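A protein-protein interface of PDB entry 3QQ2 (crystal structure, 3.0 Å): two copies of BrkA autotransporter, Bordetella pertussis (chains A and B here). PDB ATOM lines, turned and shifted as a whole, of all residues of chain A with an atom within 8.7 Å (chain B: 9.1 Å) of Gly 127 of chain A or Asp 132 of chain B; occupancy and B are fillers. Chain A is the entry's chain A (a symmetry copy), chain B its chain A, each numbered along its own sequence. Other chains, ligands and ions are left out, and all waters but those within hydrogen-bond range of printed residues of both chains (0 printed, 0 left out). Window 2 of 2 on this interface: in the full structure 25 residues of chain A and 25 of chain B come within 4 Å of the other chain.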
ATOM      1  N   ASP A  82     -25.778  -4.146   3.577  1.00  0.00           N
ATOM      2  CA  ASP A  82     -24.880  -4.987   4.396  1.00  0.00           C
ATOM      3  C   ASP A  82     -23.378  -4.592   4.452  1.00  0.00           C
ATOM      4  O   ASP A  82     -22.984  -3.588   5.070  1.00  0.00           O
ATOM      5  CB  ASP A  82     -25.046  -6.467   3.948  1.00  0.00           C
ATOM      6  CG  ASP A  82     -26.438  -6.756   3.310  1.00  0.00           C
ATOM      7  OD1 ASP A  82     -27.486  -6.597   4.001  1.00  0.00           O
ATOM      8  OD2 ASP A  82     -26.479  -7.140   2.113  1.00  0.00           O
ATOM      9  N   ASN A 120     -17.748 -10.037   5.903  1.00  0.00           N
ATOM     10  CA  ASN A 120     -18.353  -9.175   6.914  1.00  0.00           C
ATOM     11  C   ASN A 120     -19.781  -8.726   6.605  1.00  0.00           C
ATOM     12  O   ASN A 120     -19.978  -7.759   5.883  1.00  0.00           O
ATOM     13  CB  ASN A 120     -17.465  -7.966   7.148  1.00  0.00           C
ATOM     14  CG  ASN A 120     -17.773  -7.298   8.439  1.00  0.00           C
ATOM     15  OD1 ASN A 120     -18.936  -7.082   8.760  1.00  0.00           O
ATOM     16  ND2 ASN A 120     -16.741  -6.980   9.215  1.00  0.00           N
ATOM     17  N   ILE A 121     -20.776  -9.403   7.166  1.00  0.00           N
ATOM     18  CA  ILE A 121     -22.152  -9.174   6.732  1.00  0.00           C
ATOM     19  C   ILE A 121     -22.986  -8.415   7.760  1.00  0.00           C
ATOM     20  O   ILE A 121     -22.504  -8.070   8.836  1.00  0.00           O
ATOM     21  CB  ILE A 121     -22.862 -10.502   6.341  1.00  0.00           C
ATOM     22  CG1 ILE A 121     -21.963 -11.373   5.452  1.00  0.00           C
ATOM     23  CG2 ILE A 121     -24.190 -10.237   5.627  1.00  0.00           C
ATOM     24  CD1 ILE A 121     -21.547 -10.729   4.130  1.00  0.00           C
ATOM     25  N   ALA A 122     -24.229  -8.124   7.383  1.00  0.00           N
ATOM     26  CA  ALA A 122     -25.260  -7.591   8.275  1.00  0.00           C
ATOM     27  C   ALA A 122     -26.612  -8.155   7.821  1.00  0.00           C
ATOM     28  O   ALA A 122     -26.804  -8.453   6.633  1.00  0.00           O
ATOM     29  CB  ALA A 122     -25.264  -6.059   8.267  1.00  0.00           C
ATOM     30  N   GLY A 123     -27.533  -8.311   8.770  1.00  0.00           N
ATOM     31  CA  GLY A 123     -28.787  -9.009   8.512  1.00  0.00           C
ATOM     32  C   GLY A 123     -30.023  -8.140   8.413  1.00  0.00           C
ATOM     33  O   GLY A 123     -31.137  -8.664   8.474  1.00  0.00           O
ATOM     34  N   THR A 124     -29.836  -6.823   8.256  1.00  0.00           N
ATOM     35  CA  THR A 124     -30.938  -5.815   8.205  1.00  0.00           C
ATOM     36  C   THR A 124     -31.879  -5.805   9.438  1.00  0.00           C
ATOM     37  O   THR A 124     -32.642  -4.848   9.647  1.00  0.00           O
ATOM     38  CB  THR A 124     -31.796  -5.859   6.882  1.00  0.00           C
ATOM     39  OG1 THR A 124     -32.888  -6.784   7.029  1.00  0.00           O
ATOM     40  CG2 THR A 124     -30.939  -6.198   5.628  1.00  0.00           C
ATOM     41  N   ASP A 125     -31.820  -6.883  10.226  1.00  0.00           N
ATOM     42  CA  ASP A 125     -32.467  -6.979  11.541  1.00  0.00           C
ATOM     43  C   ASP A 125     -31.564  -6.371  12.636  1.00  0.00           C
ATOM     44  O   ASP A 125     -31.974  -6.199  13.794  1.00  0.00           O
ATOM     45  CB  ASP A 125     -32.766  -8.455  11.880  1.00  0.00           C
ATOM     46  CG  ASP A 125     -33.753  -9.106  10.910  1.00  0.00           C
ATOM     47  OD1 ASP A 125     -34.928  -9.302  11.313  1.00  0.00           O
ATOM     48  OD2 ASP A 125     -33.353  -9.421   9.758  1.00  0.00           O
ATOM     49  N   GLY A 126     -30.331  -6.051  12.244  1.00  0.00           N
ATOM     50  CA  GLY A 126     -29.321  -5.523  13.151  1.00  0.00           C
ATOM     51  C   GLY A 126     -28.165  -6.491  13.330  1.00  0.00           C
ATOM     52  O   GLY A 126     -27.096  -6.098  13.812  1.00  0.00           O
ATOM     53  N   GLY A 127     -28.383  -7.749  12.934  1.00  0.00           N
ATOM     54  CA  GLY A 127     -27.448  -8.839  13.198  1.00  0.00           C
ATOM     55  C   GLY A 127     -26.198  -8.744  12.365  1.00  0.00           C
ATOM     56  O   GLY A 127     -26.284  -8.520  11.167  1.00  0.00           O
ATOM     57  N   ARG A 128     -25.040  -8.909  12.999  1.00  0.00           N
ATOM     58  CA  ARG A 128     -23.754  -8.799  12.320  1.00  0.00           C
ATOM     59  C   ARG A 128     -22.937 -10.084  12.490  1.00  0.00           C
ATOM     60  O   ARG A 128     -22.543 -10.450  13.592  1.00  0.00           O
ATOM     61  CB  ARG A 128     -22.980  -7.583  12.850  1.00  0.00           C
ATOM     62  CG  ARG A 128     -22.152  -6.800  11.790  1.00  0.00           C
ATOM     63  CD  ARG A 128     -22.896  -5.544  11.214  1.00  0.00           C
ATOM     64  NE  ARG A 128     -23.343  -4.628  12.275  1.00  0.00           N
ATOM     65  CZ  ARG A 128     -24.618  -4.418  12.631  1.00  0.00           C
ATOM     66  NH1 ARG A 128     -25.619  -5.029  11.997  1.00  0.00           N
ATOM     67  NH2 ARG A 128     -24.905  -3.577  13.619  1.00  0.00           N
ATOM     68  N   VAL A 129     -22.695 -10.779  11.393  1.00  0.00           N
ATOM     69  CA  VAL A 129     -21.861 -11.968  11.410  1.00  0.00           C
ATOM     70  C   VAL A 129     -20.510 -11.672  10.752  1.00  0.00           C
ATOM     71  O   VAL A 129     -20.462 -11.078   9.680  1.00  0.00           O
ATOM     72  CB  VAL A 129     -22.577 -13.142  10.710  1.00  0.00           C
ATOM     73  CG1 VAL A 129     -22.618 -12.943   9.195  1.00  0.00           C
ATOM     74  CG2 VAL A 129     -21.924 -14.459  11.045  1.00  0.00           C
ATOM     75  N   THR A 130     -19.417 -12.075  11.394  1.00  0.00           N
ATOM     76  CA  THR A 130     -18.052 -11.883  10.848  1.00  0.00           C
ATOM     77  C   THR A 130     -17.353 -13.201  10.516  1.00  0.00           C
ATOM     78  O   THR A 130     -17.487 -14.158  11.242  1.00  0.00           O
ATOM     79  CB  THR A 130     -17.195 -11.040  11.807  1.00  0.00           C
ATOM     80  OG1 THR A 130     -17.198  -9.684  11.364  1.00  0.00           O
ATOM     81  CG2 THR A 130     -15.752 -11.554  11.907  1.00  0.00           C
ATOM     82  N   LEU A 178     -25.314 -22.337  16.996  1.00  0.00           N
ATOM     83  CA  LEU A 178     -24.993 -21.703  15.723  1.00  0.00           C
ATOM     84  C   LEU A 178     -24.254 -22.593  14.728  1.00  0.00           C
ATOM     85  O   LEU A 178     -23.365 -23.351  15.102  1.00  0.00           O
ATOM     86  CB  LEU A 178     -24.202 -20.417  15.993  1.00  0.00           C
ATOM     87  CG  LEU A 178     -23.335 -19.763  14.921  1.00  0.00           C
ATOM     88  CD1 LEU A 178     -23.433 -18.269  15.051  1.00  0.00           C
ATOM     89  CD2 LEU A 178     -21.886 -20.235  15.043  1.00  0.00           C
ATOM     90  N   LYS B  86     -21.675 -15.025  24.768  1.00  0.00           N
ATOM     91  CA  LYS B  86     -22.265 -14.355  25.922  1.00  0.00           C
ATOM     92  C   LYS B  86     -23.755 -14.256  25.595  1.00  0.00           C
ATOM     93  O   LYS B  86     -24.126 -14.201  24.420  1.00  0.00           O
ATOM     94  CB  LYS B  86     -21.688 -12.954  26.063  1.00  0.00           C
ATOM     95  CG  LYS B  86     -20.187 -12.888  26.287  1.00  0.00           C
ATOM     96  CD  LYS B  86     -19.877 -12.899  27.771  1.00  0.00           C
ATOM     97  CE  LYS B  86     -18.464 -13.359  28.075  1.00  0.00           C
ATOM     98  NZ  LYS B  86     -17.540 -12.216  28.202  1.00  0.00           N
ATOM     99  N   LYS B  88     -27.422 -12.179  26.857  1.00  0.00           N
ATOM    100  CA  LYS B  88     -28.144 -11.251  27.737  1.00  0.00           C
ATOM    101  C   LYS B  88     -29.604 -11.217  27.352  1.00  0.00           C
ATOM    102  O   LYS B  88     -29.930 -11.337  26.173  1.00  0.00           O
ATOM    103  CB  LYS B  88     -27.583  -9.851  27.640  1.00  0.00           C
ATOM    104  CG  LYS B  88     -26.114  -9.727  27.948  1.00  0.00           C
ATOM    105  CD  LYS B  88     -25.496  -8.679  26.994  1.00  0.00           C
ATOM    106  CE  LYS B  88     -25.389  -7.284  27.621  1.00  0.00           C
ATOM    107  NZ  LYS B  88     -24.164  -7.180  28.497  1.00  0.00           N
ATOM    108  N   TYR B 115     -33.494 -12.315  23.454  1.00  0.00           N
ATOM    109  CA  TYR B 115     -32.084 -12.457  23.784  1.00  0.00           C
ATOM    110  C   TYR B 115     -31.097 -11.780  22.827  1.00  0.00           C
ATOM    111  O   TYR B 115     -31.453 -11.388  21.722  1.00  0.00           O
ATOM    112  CB  TYR B 115     -31.770 -13.921  24.160  1.00  0.00           C
ATOM    113  CG  TYR B 115     -32.469 -14.210  25.460  1.00  0.00           C
ATOM    114  CD1 TYR B 115     -33.653 -14.951  25.507  1.00  0.00           C
ATOM    115  CD2 TYR B 115     -32.002 -13.620  26.652  1.00  0.00           C
ATOM    116  CE1 TYR B 115     -34.340 -15.141  26.745  1.00  0.00           C
ATOM    117  CE2 TYR B 115     -32.664 -13.796  27.882  1.00  0.00           C
ATOM    118  CZ  TYR B 115     -33.834 -14.550  27.928  1.00  0.00           C
ATOM    119  OH  TYR B 115     -34.465 -14.696  29.155  1.00  0.00           O
ATOM    120  N   ASP B 116     -29.879 -11.594  23.311  1.00  0.00           N
ATOM    121  CA  ASP B 116     -28.811 -10.927  22.601  1.00  0.00           C
ATOM    122  C   ASP B 116     -27.550 -11.711  22.768  1.00  0.00           C
ATOM    123  O   ASP B 116     -26.954 -11.717  23.844  1.00  0.00           O
ATOM    124  CB  ASP B 116     -28.543  -9.592  23.244  1.00  0.00           C
ATOM    125  CG  ASP B 116     -29.111  -8.458  22.476  1.00  0.00           C
ATOM    126  OD1 ASP B 116     -30.238  -8.591  21.942  1.00  0.00           O
ATOM    127  OD2 ASP B 116     -28.417  -7.417  22.425  1.00  0.00           O
ATOM    128  N   GLN B 117     -27.116 -12.359  21.709  1.00  0.00           N
ATOM    129  CA  GLN B 117     -25.952 -13.199  21.816  1.00  0.00           C
ATOM    130  C   GLN B 117     -24.849 -12.651  20.970  1.00  0.00           C
ATOM    131  O   GLN B 117     -25.094 -12.211  19.860  1.00  0.00           O
ATOM    132  CB  GLN B 117     -26.302 -14.622  21.415  1.00  0.00           C
ATOM    133  CG  GLN B 117     -27.634 -14.727  20.696  1.00  0.00           C
ATOM    134  CD  GLN B 117     -28.512 -15.854  21.229  1.00  0.00           C
ATOM    135  OE1 GLN B 117     -29.744 -15.706  21.308  1.00  0.00           O
ATOM    136  NE2 GLN B 117     -27.885 -16.995  21.599  1.00  0.00           N
ATOM    137  N   GLN B 118     -23.646 -12.634  21.523  1.00  0.00           N
ATOM    138  CA  GLN B 118     -22.465 -12.330  20.748  1.00  0.00           C
ATOM    139  C   GLN B 118     -21.602 -13.573  20.753  1.00  0.00           C
ATOM    140  O   GLN B 118     -20.826 -13.771  21.671  1.00  0.00           O
ATOM    141  CB  GLN B 118     -21.668 -11.176  21.356  1.00  0.00           C
ATOM    142  CG  GLN B 118     -22.467  -9.993  21.869  1.00  0.00           C
ATOM    143  CD  GLN B 118     -21.772  -9.319  23.063  1.00  0.00           C
ATOM    144  OE1 GLN B 118     -22.091  -8.175  23.431  1.00  0.00           O
ATOM    145  NE2 GLN B 118     -20.816 -10.033  23.680  1.00  0.00           N
ATOM    146  N   TYR B 119     -21.726 -14.421  19.742  1.00  0.00           N
ATOM    147  CA  TYR B 119     -20.878 -15.609  19.683  1.00  0.00           C
ATOM    148  C   TYR B 119     -19.517 -15.279  19.128  1.00  0.00           C
ATOM    149  O   TYR B 119     -19.358 -14.322  18.366  1.00  0.00           O
ATOM    150  CB  TYR B 119     -21.547 -16.747  18.906  1.00  0.00           C
ATOM    151  CG  TYR B 119     -22.445 -17.573  19.802  1.00  0.00           C
ATOM    152  CD1 TYR B 119     -22.035 -18.816  20.284  1.00  0.00           C
ATOM    153  CD2 TYR B 119     -23.690 -17.079  20.213  1.00  0.00           C
ATOM    154  CE1 TYR B 119     -22.857 -19.558  21.133  1.00  0.00           C
ATOM    155  CE2 TYR B 119     -24.518 -17.812  21.062  1.00  0.00           C
ATOM    156  CZ  TYR B 119     -24.100 -19.044  21.512  1.00  0.00           C
ATOM    157  OH  TYR B 119     -24.931 -19.743  22.347  1.00  0.00           O
ATOM    158  N   ASN B 120     -18.526 -16.059  19.529  1.00  0.00           N
ATOM    159  CA  ASN B 120     -17.169 -15.833  19.042  1.00  0.00           C
ATOM    160  C   ASN B 120     -16.297 -17.087  18.963  1.00  0.00           C
ATOM    161  O   ASN B 120     -15.710 -17.490  19.957  1.00  0.00           O
ATOM    162  CB  ASN B 120     -16.490 -14.780  19.897  1.00  0.00           C
ATOM    163  CG  ASN B 120     -15.311 -14.189  19.212  1.00  0.00           C
ATOM    164  OD1 ASN B 120     -14.500 -14.913  18.646  1.00  0.00           O
ATOM    165  ND2 ASN B 120     -15.206 -12.863  19.228  1.00  0.00           N
ATOM    166  N   VAL B 129     -14.812 -17.097  13.181  1.00  0.00           N
ATOM    167  CA  VAL B 129     -16.134 -16.614  12.825  1.00  0.00           C
ATOM    168  C   VAL B 129     -16.745 -15.841  13.998  1.00  0.00           C
ATOM    169  O   VAL B 129     -16.704 -16.305  15.132  1.00  0.00           O
ATOM    170  CB  VAL B 129     -17.042 -17.785  12.396  1.00  0.00           C
ATOM    171  CG1 VAL B 129     -17.454 -18.638  13.596  1.00  0.00           C
ATOM    172  CG2 VAL B 129     -18.264 -17.291  11.665  1.00  0.00           C
ATOM    173  N   THR B 130     -17.302 -14.663  13.729  1.00  0.00           N
ATOM    174  CA  THR B 130     -17.959 -13.834  14.767  1.00  0.00           C
ATOM    175  C   THR B 130     -19.464 -13.677  14.540  1.00  0.00           C
ATOM    176  O   THR B 130     -19.895 -13.539  13.419  1.00  0.00           O
ATOM    177  CB  THR B 130     -17.281 -12.458  14.876  1.00  0.00           C
ATOM    178  OG1 THR B 130     -16.355 -12.480  15.961  1.00  0.00           O
ATOM    179  CG2 THR B 130     -18.293 -11.321  15.076  1.00  0.00           C
ATOM    180  N   ALA B 131     -20.256 -13.707  15.596  1.00  0.00           N
ATOM    181  CA  ALA B 131     -21.695 -13.547  15.435  1.00  0.00           C
ATOM    182  C   ALA B 131     -22.338 -12.634  16.478  1.00  0.00           C
ATOM    183  O   ALA B 131     -21.874 -12.511  17.613  1.00  0.00           O
ATOM    184  CB  ALA B 131     -22.376 -14.885  15.431  1.00  0.00           C
ATOM    185  N   ASP B 132     -23.440 -12.019  16.082  1.00  0.00           N
ATOM    186  CA  ASP B 132     -24.096 -11.027  16.899  1.00  0.00           C
ATOM    187  C   ASP B 132     -25.552 -10.908  16.481  1.00  0.00           C
ATOM    188  O   ASP B 132     -25.828 -10.407  15.396  1.00  0.00           O
ATOM    189  CB  ASP B 132     -23.403  -9.708  16.642  1.00  0.00           C
ATOM    190  CG  ASP B 132     -22.958  -9.054  17.894  1.00  0.00           C
ATOM    191  OD1 ASP B 132     -23.805  -8.915  18.793  1.00  0.00           O
ATOM    192  OD2 ASP B 132     -21.765  -8.683  17.981  1.00  0.00           O
ATOM    193  N   TYR B 133     -26.488 -11.357  17.317  1.00  0.00           N
ATOM    194  CA  TYR B 133     -27.910 -11.300  16.934  1.00  0.00           C
ATOM    195  C   TYR B 133     -28.923 -11.401  18.078  1.00  0.00           C
ATOM    196  O   TYR B 133     -28.607 -11.904  19.154  1.00  0.00           O
ATOM    197  CB  TYR B 133     -28.211 -12.392  15.924  1.00  0.00           C
ATOM    198  CG  TYR B 133     -27.832 -13.752  16.430  1.00  0.00           C
ATOM    199  CD1 TYR B 133     -26.522 -14.206  16.303  1.00  0.00           C
ATOM    200  CD2 TYR B 133     -28.772 -14.585  17.044  1.00  0.00           C
ATOM    201  CE1 TYR B 133     -26.151 -15.448  16.766  1.00  0.00           C
ATOM    202  CE2 TYR B 133     -28.411 -15.823  17.518  1.00  0.00           C
ATOM    203  CZ  TYR B 133     -27.089 -16.250  17.370  1.00  0.00           C
ATOM    204  OH  TYR B 133     -26.675 -17.485  17.803  1.00  0.00           O
ATOM    205  N   ARG B 134     -30.149 -10.932  17.813  1.00  0.00           N
ATOM    206  CA  ARG B 134     -31.279 -11.052  18.746  1.00  0.00           C
ATOM    207  C   ARG B 134     -32.096 -12.286  18.401  1.00  0.00           C
ATOM    208  O   ARG B 134     -32.113 -12.730  17.261  1.00  0.00           O
ATOM    209  CB  ARG B 134     -32.180  -9.800  18.750  1.00  0.00           C
ATOM    210  CG  ARG B 134     -31.496  -8.474  19.181  1.00  0.00           C
ATOM    211  CD  ARG B 134     -32.507  -7.334  19.601  1.00  0.00           C
ATOM    212  NE  ARG B 134     -32.748  -7.248  21.059  1.00  0.00           N
ATOM    213  CZ  ARG B 134     -33.907  -7.523  21.682  1.00  0.00           C
ATOM    214  NH1 ARG B 134     -34.979  -7.900  20.974  1.00  0.00           N
ATOM    215  NH2 ARG B 134     -34.000  -7.416  23.025  1.00  0.00           N
ATOM    216  N   THR B 135     -32.771 -12.820  19.411  1.00  0.00           N
ATOM    217  CA  THR B 135     -33.526 -14.065  19.330  1.00  0.00           C
ATOM    218  C   THR B 135     -34.706 -14.000  20.294  1.00  0.00           C
ATOM    219  O   THR B 135     -34.704 -13.192  21.230  1.00  0.00           O
ATOM    220  CB  THR B 135     -32.620 -15.227  19.715  1.00  0.00           C
ATOM    221  OG1 THR B 135     -31.872 -15.614  18.565  1.00  0.00           O
ATOM    222  CG2 THR B 135     -33.419 -16.422  20.194  1.00  0.00           C
ATOM    223  N   LYS B 170     -32.550 -17.956  13.143  1.00  0.00           N
ATOM    224  CA  LYS B 170     -32.139 -16.904  12.190  1.00  0.00           C
ATOM    225  C   LYS B 170     -31.157 -17.538  11.224  1.00  0.00           C
ATOM    226  O   LYS B 170     -30.399 -18.422  11.608  1.00  0.00           O
ATOM    227  CB  LYS B 170     -31.452 -15.722  12.887  1.00  0.00           C
ATOM    228  CG  LYS B 170     -32.358 -14.536  13.181  1.00  0.00           C
ATOM    229  CD  LYS B 170     -31.590 -13.352  13.776  1.00  0.00           C
ATOM    230  CE  LYS B 170     -32.504 -12.119  13.988  1.00  0.00           C
ATOM    231  NZ  LYS B 170     -31.805 -10.921  14.605  1.00  0.00           N
ATOM    232  N   TYR B 172     -29.021 -16.267   7.344  1.00  0.00           N
ATOM    233  CA  TYR B 172     -28.781 -15.404   6.170  1.00  0.00           C
ATOM    234  C   TYR B 172     -27.754 -16.067   5.239  1.00  0.00           C
ATOM    235  O   TYR B 172     -27.512 -17.274   5.363  1.00  0.00           O
ATOM    236  CB  TYR B 172     -28.373 -13.972   6.589  1.00  0.00           C
ATOM    237  CG  TYR B 172     -27.930 -13.815   8.041  1.00  0.00           C
ATOM    238  CD1 TYR B 172     -26.710 -13.210   8.356  1.00  0.00           C
ATOM    239  CD2 TYR B 172     -28.744 -14.250   9.108  1.00  0.00           C
ATOM    240  CE1 TYR B 172     -26.302 -13.055   9.693  1.00  0.00           C
ATOM    241  CE2 TYR B 172     -28.338 -14.113  10.436  1.00  0.00           C
ATOM    242  CZ  TYR B 172     -27.118 -13.514  10.712  1.00  0.00           C
ATOM    243  OH  TYR B 172     -26.720 -13.375  12.008  1.00  0.00           O
ATOM    244  N   VAL B 180     -24.803 -19.075   7.093  1.00  0.00           N
ATOM    245  CA  VAL B 180     -24.906 -19.027   8.551  1.00  0.00           C
ATOM    246  C   VAL B 180     -26.325 -19.341   8.992  1.00  0.00           C
ATOM    247  O   VAL B 180     -27.271 -18.672   8.587  1.00  0.00           O
ATOM    248  CB  VAL B 180     -24.497 -17.646   9.119  1.00  0.00           C
ATOM    249  CG1 VAL B 180     -25.190 -16.500   8.363  1.00  0.00           C
ATOM    250  CG2 VAL B 180     -24.791 -17.566  10.617  1.00  0.00           C
ATOM    251  N   VAL B 182     -28.645 -20.089  12.539  1.00  0.00           N
ATOM    252  CA  VAL B 182     -28.903 -20.284  13.949  1.00  0.00           C
ATOM    253  C   VAL B 182     -30.138 -21.155  13.987  1.00  0.00           C
ATOM    254  O   VAL B 182     -31.131 -20.856  13.330  1.00  0.00           O
ATOM    255  CB  VAL B 182     -29.232 -18.966  14.703  1.00  0.00           C
ATOM    256  CG1 VAL B 182     -29.120 -19.197  16.197  1.00  0.00           C
ATOM    257  CG2 VAL B 182     -28.318 -17.824  14.273  1.00  0.00           C
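Val 129 of chain A touches Thr 130 of chain B, and with the chains exchanged Thr 130 of chain A touches Val 129 of chain B.
Thr 130 of chain A touches its own counterpart, Thr 130 of chain B.
3 positions are printed for both chains.
Of the 9 pairs that touch across the chains among the printed residues, 3 have their exchanged pair printed and touching as well.
Among the printed residues, pairs that only touch across the chains: Gly 127 of chain A with Asp 132 of chain B, Thr 130 of chain A with Val 129 of chain B, Val 129 of chain A with Thr 130 of chain B, Leu 178 of chain A with Ala 131 of chain B, Arg 128 of chain A with Ala 131 of chain B, Val 129 of chain A with Tyr 172 of chain B and Asp 125 of chain A with Lys 170 of chain B.
The backbone NH (N) of Thr 130 of chain B is in hydrogen-bond range of the backbone carbonyl oxygen (O) of Thr 130 of chain A (2.5 Å).
The backbone carbonyl oxygen of Asp 132 of chain B sits at hydrogen-bond distance from the backbone NH of Arg 128 of chain A, 2.9 Å away.
Of the 19 printed residues of chain B, 6 touch a printed residue of chain A.
Printed residues of chain B that touch a printed residue of chain A: Val 129, Thr 130, Ala 131, Asp 132, Lys 170 and Tyr 172.
Hydrophobic or aromatic side chains of chain B that line the printed part of chain A: Val 129, Ala 131 and Tyr 172.
Of the 13 printed residues of chain A, 6 touch a printed residue of chain B.
Among the printed residues, no Asp or Glu carboxylate lies within 4 Å of a Lys or Arg side-chain nitrogen of the other chain.
Of chain A, only Gly 127 (3.1 Å) and Arg 128 (2.9 Å) come within 4 Å of Asp 132 of chain B.
Of the printed residues of chain B, Asp 125 of chain A touches Lys 170.
Printed residues of chain B within 4 Å of Arg 128 of chain A: Ala 131 (3.6 Å) and Asp 132 (2.9 Å).
Printed residues of chain A within 4 Å of Lys 170 of chain B: Asp 125.
Of the printed residues of chain A, Val 129 of chain B touches Thr 130.
Of the printed residues of chain B, Leu 178 of chain A touches Ala 131.
Arg 134 of chain B touches none of the printed residues of chain A.
Gly 123 of chain A touches none of the printed residues of chain B.
The nearest residue of chain B that does not touch Gly 127 of chain A is Tyr 133 of chain B (4.5 Å).
The nearest residue of chain A that does not touch Asp 132 of chain B is Gly 126 of chain A (4.8 Å).
The nearest printed residue of chain A that does not touch Lys 170 of chain B is Gly 127 of chain A (5.0 Å).
The backbone carbonyl oxygen (O) of Arg 134 of chain B sits at hydrogen-bond distance from the side-chain amino group (NZ) of Lys 170 of chain B.
The backbone carbonyl oxygen of Gly 126 of chain A is in hydrogen-bond range of the guanidinium group of Arg 128 of chain A (2.6 Å).
The backbone NH (N) of Tyr 119 of chain B lies within hydrogen-bond range of the backbone carbonyl oxygen (O) of Ala 131 of chain B (2.9 Å).
O of Gly 123 of chain A lies close to OD2 of Asp 125 of chain A.
The backbone NH (N) of Ile 121 of chain A sits at hydrogen-bond distance from the backbone carbonyl oxygen (O) of Val 129 of chain A, 3.0 Å away.
The backbone NH of Val 182 of chain B lies within hydrogen-bond range of the backbone carbonyl oxygen of Lys 170 of chain B (2.6 Å).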
